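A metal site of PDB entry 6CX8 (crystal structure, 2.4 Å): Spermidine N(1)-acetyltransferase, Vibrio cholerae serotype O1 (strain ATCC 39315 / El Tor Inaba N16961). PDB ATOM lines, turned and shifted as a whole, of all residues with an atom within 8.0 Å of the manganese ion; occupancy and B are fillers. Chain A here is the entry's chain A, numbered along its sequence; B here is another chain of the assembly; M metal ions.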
ATOM      1  N   PHE A  35      12.704  18.265  20.102  1.00  0.00           N
ATOM      2  CA  PHE A  35      12.579  18.732  18.690  1.00  0.00           C
ATOM      3  C   PHE A  35      13.157  20.122  18.467  1.00  0.00           C
ATOM      4  O   PHE A  35      12.612  20.946  17.777  1.00  0.00           O
ATOM      5  CB  PHE A  35      11.176  18.552  18.102  1.00  0.00           C
ATOM      6  CG  PHE A  35      10.813  17.095  17.958  1.00  0.00           C
ATOM      7  CD1 PHE A  35      10.465  16.370  19.105  1.00  0.00           C
ATOM      8  CD2 PHE A  35      10.870  16.406  16.710  1.00  0.00           C
ATOM      9  CE1 PHE A  35      10.132  15.026  19.002  1.00  0.00           C
ATOM     10  CE2 PHE A  35      10.525  15.090  16.617  1.00  0.00           C
ATOM     11  CZ  PHE A  35      10.200  14.383  17.741  1.00  0.00           C
ATOM     12  N   GLU A  36      14.338  20.305  19.029  1.00  0.00           N
ATOM     13  CA  GLU A  36      15.116  21.557  18.903  1.00  0.00           C
ATOM     14  C   GLU A  36      14.511  22.726  19.650  1.00  0.00           C
ATOM     15  O   GLU A  36      15.044  23.762  19.551  1.00  0.00           O
ATOM     16  CB  GLU A  36      15.505  21.864  17.428  1.00  0.00           C
ATOM     17  CG  GLU A  36      16.110  20.630  16.748  1.00  0.00           C
ATOM     18  CD  GLU A  36      16.818  20.847  15.396  1.00  0.00           C
ATOM     19  OE1 GLU A  36      16.959  19.865  14.656  1.00  0.00           O
ATOM     20  OE2 GLU A  36      17.342  21.919  15.060  1.00  0.00           O
ATOM     21  N   ALA A  57      11.824  13.219  12.864  1.00  0.00           N
ATOM     22  CA  ALA A  57      13.187  13.757  12.984  1.00  0.00           C
ATOM     23  C   ALA A  57      13.869  13.389  14.280  1.00  0.00           C
ATOM     24  O   ALA A  57      15.044  13.584  14.406  1.00  0.00           O
ATOM     25  CB  ALA A  57      13.187  15.225  12.756  1.00  0.00           C
ATOM     26  N   GLU A  58      13.132  12.860  15.246  1.00  0.00           N
ATOM     27  CA  GLU A  58      13.711  12.428  16.519  1.00  0.00           C
ATOM     28  C   GLU A  58      12.960  11.196  16.944  1.00  0.00           C
ATOM     29  O   GLU A  58      11.820  11.050  16.646  1.00  0.00           O
ATOM     30  CB  GLU A  58      13.720  13.520  17.632  1.00  0.00           C
ATOM     31  CG  GLU A  58      14.337  14.835  17.202  1.00  0.00           C
ATOM     32  CD  GLU A  58      14.498  15.904  18.269  1.00  0.00           C
ATOM     33  OE1 GLU A  58      15.236  16.905  18.021  1.00  0.00           O
ATOM     34  OE2 GLU A  58      13.921  15.749  19.329  1.00  0.00           O
ATOM     35  N   ILE A  77      18.420  12.241  17.425  1.00  0.00           N
ATOM     36  CA  ILE A  77      17.926  13.497  16.880  1.00  0.00           C
ATOM     37  C   ILE A  77      18.564  13.847  15.588  1.00  0.00           C
ATOM     38  O   ILE A  77      19.458  13.139  15.145  1.00  0.00           O
ATOM     39  CB  ILE A  77      18.062  14.633  17.885  1.00  0.00           C
ATOM     40  CG1 ILE A  77      19.469  14.960  18.190  1.00  0.00           C
ATOM     41  CG2 ILE A  77      17.410  14.235  19.200  1.00  0.00           C
ATOM     42  CD1 ILE A  77      19.600  16.083  19.224  1.00  0.00           C
ATOM     43  N   GLU A  78      18.096  14.936  14.948  1.00  0.00           N
ATOM     44  CA  GLU A  78      18.586  15.427  13.675  1.00  0.00           C
ATOM     45  C   GLU A  78      18.550  14.271  12.652  1.00  0.00           C
ATOM     46  O   GLU A  78      19.322  14.210  11.783  1.00  0.00           O
ATOM     47  CB  GLU A  78      20.061  15.928  13.788  1.00  0.00           C
ATOM     48  CG  GLU A  78      20.196  17.129  14.759  1.00  0.00           C
ATOM     49  CD  GLU A  78      19.667  18.426  14.221  1.00  0.00           C
ATOM     50  OE1 GLU A  78      19.835  19.458  14.849  1.00  0.00           O
ATOM     51  OE2 GLU A  78      19.082  18.535  13.127  1.00  0.00           O
ATOM     52  N   ILE A  79      17.629  13.341  12.777  1.00  0.00           N
ATOM     53  CA  ILE A  79      17.582  12.230  11.850  1.00  0.00           C
ATOM     54  C   ILE A  79      17.250  12.745  10.462  1.00  0.00           C
ATOM     55  O   ILE A  79      16.356  13.545  10.324  1.00  0.00           O
ATOM     56  CB  ILE A  79      16.542  11.211  12.256  1.00  0.00           C
ATOM     57  CG1 ILE A  79      16.655  10.835  13.686  1.00  0.00           C
ATOM     58  CG2 ILE A  79      16.608  10.011  11.337  1.00  0.00           C
ATOM     59  CD1 ILE A  79      15.574   9.875  14.131  1.00  0.00           C
ATOM     60  N   GLU A  87      22.081  12.077  15.229  1.00  0.00           N
ATOM     61  CA  GLU A  87      22.845  12.380  16.384  1.00  0.00           C
ATOM     62  C   GLU A  87      22.245  11.522  17.493  1.00  0.00           C
ATOM     63  O   GLU A  87      21.074  11.343  17.598  1.00  0.00           O
ATOM     64  CB  GLU A  87      22.750  13.842  16.713  1.00  0.00           C
ATOM     65  CG  GLU A  87      23.522  14.177  17.956  1.00  0.00           C
ATOM     66  CD  GLU A  87      23.540  15.664  18.317  1.00  0.00           C
ATOM     67  OE1 GLU A  87      23.236  16.539  17.456  1.00  0.00           O
ATOM     68  OE2 GLU A  87      23.910  15.893  19.487  1.00  0.00           O
ATOM     69  N   TYR A 123      26.399   9.995  14.916  1.00  0.00           N
ATOM     70  CA  TYR A 123      27.386  10.816  15.574  1.00  0.00           C
ATOM     71  C   TYR A 123      26.890  11.308  16.936  1.00  0.00           C
ATOM     72  O   TYR A 123      25.707  11.159  17.270  1.00  0.00           O
ATOM     73  CB  TYR A 123      27.784  11.992  14.667  1.00  0.00           C
ATOM     74  CG  TYR A 123      26.690  12.944  14.308  1.00  0.00           C
ATOM     75  CD1 TYR A 123      25.895  12.723  13.207  1.00  0.00           C
ATOM     76  CD2 TYR A 123      26.493  14.097  15.053  1.00  0.00           C
ATOM     77  CE1 TYR A 123      24.909  13.637  12.850  1.00  0.00           C
ATOM     78  CE2 TYR A 123      25.496  15.007  14.704  1.00  0.00           C
ATOM     79  CZ  TYR A 123      24.699  14.775  13.621  1.00  0.00           C
ATOM     80  OH  TYR A 123      23.746  15.718  13.308  1.00  0.00           O
ATOM     81  N   PHE B  35      13.781  24.965   6.797  1.00  0.00           N
ATOM     82  CA  PHE B  35      13.546  24.540   8.205  1.00  0.00           C
ATOM     83  C   PHE B  35      13.712  23.033   8.388  1.00  0.00           C
ATOM     84  O   PHE B  35      12.972  22.375   9.058  1.00  0.00           O
ATOM     85  CB  PHE B  35      12.222  25.117   8.772  1.00  0.00           C
ATOM     86  CG  PHE B  35      12.300  26.619   8.911  1.00  0.00           C
ATOM     87  CD1 PHE B  35      12.166  27.399   7.792  1.00  0.00           C
ATOM     88  CD2 PHE B  35      12.586  27.270  10.180  1.00  0.00           C
ATOM     89  CE1 PHE B  35      12.267  28.794   7.893  1.00  0.00           C
ATOM     90  CE2 PHE B  35      12.648  28.654  10.239  1.00  0.00           C
ATOM     91  CZ  PHE B  35      12.522  29.395   9.096  1.00  0.00           C
ATOM     92  N   GLU B  36      14.775  22.510   7.801  1.00  0.00           N
ATOM     93  CA  GLU B  36      15.197  21.130   7.867  1.00  0.00           C
ATOM     94  C   GLU B  36      14.245  20.164   7.170  1.00  0.00           C
ATOM     95  O   GLU B  36      14.431  18.970   7.248  1.00  0.00           O
ATOM     96  CB  GLU B  36      15.543  20.682   9.286  1.00  0.00           C
ATOM     97  CG  GLU B  36      16.415  21.694  10.061  1.00  0.00           C
ATOM     98  CD  GLU B  36      16.883  21.223  11.456  1.00  0.00           C
ATOM     99  OE1 GLU B  36      17.329  22.121  12.172  1.00  0.00           O
ATOM    100  OE2 GLU B  36      16.990  19.994  11.843  1.00  0.00           O
ATOM    101  N   ALA B  57      14.482  30.080  14.018  1.00  0.00           N
ATOM    102  CA  ALA B  57      15.633  29.170  13.951  1.00  0.00           C
ATOM    103  C   ALA B  57      16.374  29.325  12.590  1.00  0.00           C
ATOM    104  O   ALA B  57      17.433  28.765  12.465  1.00  0.00           O
ATOM    105  CB  ALA B  57      15.175  27.777  14.142  1.00  0.00           C
ATOM    106  N   GLU B  58      15.810  30.025  11.611  1.00  0.00           N
ATOM    107  CA  GLU B  58      16.482  30.259  10.366  1.00  0.00           C
ATOM    108  C   GLU B  58      16.107  31.645   9.908  1.00  0.00           C
ATOM    109  O   GLU B  58      15.011  32.115  10.179  1.00  0.00           O
ATOM    110  CB  GLU B  58      16.152  29.221   9.250  1.00  0.00           C
ATOM    111  CG  GLU B  58      16.364  27.773   9.700  1.00  0.00           C
ATOM    112  CD  GLU B  58      16.180  26.696   8.648  1.00  0.00           C
ATOM    113  OE1 GLU B  58      16.644  25.514   8.881  1.00  0.00           O
ATOM    114  OE2 GLU B  58      15.651  27.011   7.592  1.00  0.00           O
ATOM    115  N   ILE B  77      21.050  29.135   9.551  1.00  0.00           N
ATOM    116  CA  ILE B  77      20.195  28.047  10.028  1.00  0.00           C
ATOM    117  C   ILE B  77      20.736  27.476  11.317  1.00  0.00           C
ATOM    118  O   ILE B  77      21.786  27.883  11.757  1.00  0.00           O
ATOM    119  CB  ILE B  77      19.983  26.939   8.996  1.00  0.00           C
ATOM    120  CG1 ILE B  77      21.227  26.235   8.654  1.00  0.00           C
ATOM    121  CG2 ILE B  77      19.476  27.520   7.727  1.00  0.00           C
ATOM    122  CD1 ILE B  77      20.955  25.042   7.732  1.00  0.00           C
ATOM    123  N   GLU B  78      19.985  26.585  11.937  1.00  0.00           N
ATOM    124  CA  GLU B  78      20.278  25.965  13.271  1.00  0.00           C
ATOM    125  C   GLU B  78      20.575  27.070  14.242  1.00  0.00           C
ATOM    126  O   GLU B  78      21.359  26.916  15.111  1.00  0.00           O
ATOM    127  CB  GLU B  78      21.445  25.019  13.152  1.00  0.00           C
ATOM    128  CG  GLU B  78      21.265  23.835  12.202  1.00  0.00           C
ATOM    129  CD  GLU B  78      20.298  22.764  12.674  1.00  0.00           C
ATOM    130  OE1 GLU B  78      19.974  21.854  11.926  1.00  0.00           O
ATOM    131  OE2 GLU B  78      19.711  22.827  13.725  1.00  0.00           O
ATOM    132  N   ILE B  79      19.966  28.234  14.114  1.00  0.00           N
ATOM    133  CA  ILE B  79      20.246  29.324  15.047  1.00  0.00           C
ATOM    134  C   ILE B  79      19.820  28.923  16.450  1.00  0.00           C
ATOM    135  O   ILE B  79      18.799  28.390  16.605  1.00  0.00           O
ATOM    136  CB  ILE B  79      19.514  30.562  14.668  1.00  0.00           C
ATOM    137  CG1 ILE B  79      19.781  30.913  13.229  1.00  0.00           C
ATOM    138  CG2 ILE B  79      19.974  31.711  15.550  1.00  0.00           C
ATOM    139  CD1 ILE B  79      19.042  32.142  12.732  1.00  0.00           C
ATOM    140  N   GLU B  87      24.622  28.178  11.635  1.00  0.00           N
ATOM    141  CA  GLU B  87      25.221  27.681  10.486  1.00  0.00           C
ATOM    142  C   GLU B  87      24.905  28.634   9.361  1.00  0.00           C
ATOM    143  O   GLU B  87      23.805  29.156   9.252  1.00  0.00           O
ATOM    144  CB  GLU B  87      24.719  26.311  10.170  1.00  0.00           C
ATOM    145  CG  GLU B  87      25.350  25.711   8.945  1.00  0.00           C
ATOM    146  CD  GLU B  87      24.845  24.320   8.585  1.00  0.00           C
ATOM    147  OE1 GLU B  87      24.328  23.612   9.473  1.00  0.00           O
ATOM    148  OE2 GLU B  87      25.108  23.926   7.434  1.00  0.00           O
ATOM    149  N   TYR B 123      29.366  28.965  11.976  1.00  0.00           N
ATOM    150  CA  TYR B 123      30.064  27.874  11.345  1.00  0.00           C
ATOM    151  C   TYR B 123      29.421  27.553   9.981  1.00  0.00           C
ATOM    152  O   TYR B 123      28.319  28.019   9.647  1.00  0.00           O
ATOM    153  CB  TYR B 123      30.116  26.654  12.248  1.00  0.00           C
ATOM    154  CG  TYR B 123      28.778  26.066  12.617  1.00  0.00           C
ATOM    155  CD1 TYR B 123      28.062  26.537  13.712  1.00  0.00           C
ATOM    156  CD2 TYR B 123      28.238  25.002  11.880  1.00  0.00           C
ATOM    157  CE1 TYR B 123      26.877  25.957  14.070  1.00  0.00           C
ATOM    158  CE2 TYR B 123      27.028  24.456  12.214  1.00  0.00           C
ATOM    159  CZ  TYR B 123      26.332  24.934  13.305  1.00  0.00           C
ATOM    160  OH  TYR B 123      25.091  24.388  13.631  1.00  0.00           O
HETATM  161 MN    MN M   1      18.594  20.847  13.483  1.00  0.00          MN
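Within 4 Å of the manganese ion: Glu 36 of chain A, Glu 78 of chain A, Glu 36 of chain B and Glu 78 of chain B. The nearest printed residue that does not touch the manganese ion is Glu 58 of chain B (6.8 Å).
The backbone NH of Glu 78 of chain B lies within hydrogen-bond range of the backbone carbonyl oxygen of Ala 57 of chain B (3.4 Å). N of Glu 78 of chain A sits at hydrogen-bond distance from O of Ala 57 of chain A (3.4 Å).
OE1 of Glu 36 of chain B binds the manganese ion (2.2 Å). OE1 of Glu 36 of chain A binds the manganese ion (2.2 Å). The side-chain carboxylate (OE2) of Glu 36 of chain A binds the manganese ion (2.3 Å). OE2 of Glu 78 of chain B is bound to the manganese ion (2.3 Å). OE1 of Glu 78 of chain A is bound to the manganese ion (2.3 Å). OE1 of Glu 78 of chain B is bound to the manganese ion (2.3 Å). The manganese ion is bound by OE2 of Glu 78 of chain A, 2.4 Å away. The manganese ion is bound by OE2 of Glu 36 of chain B (2.4 Å).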
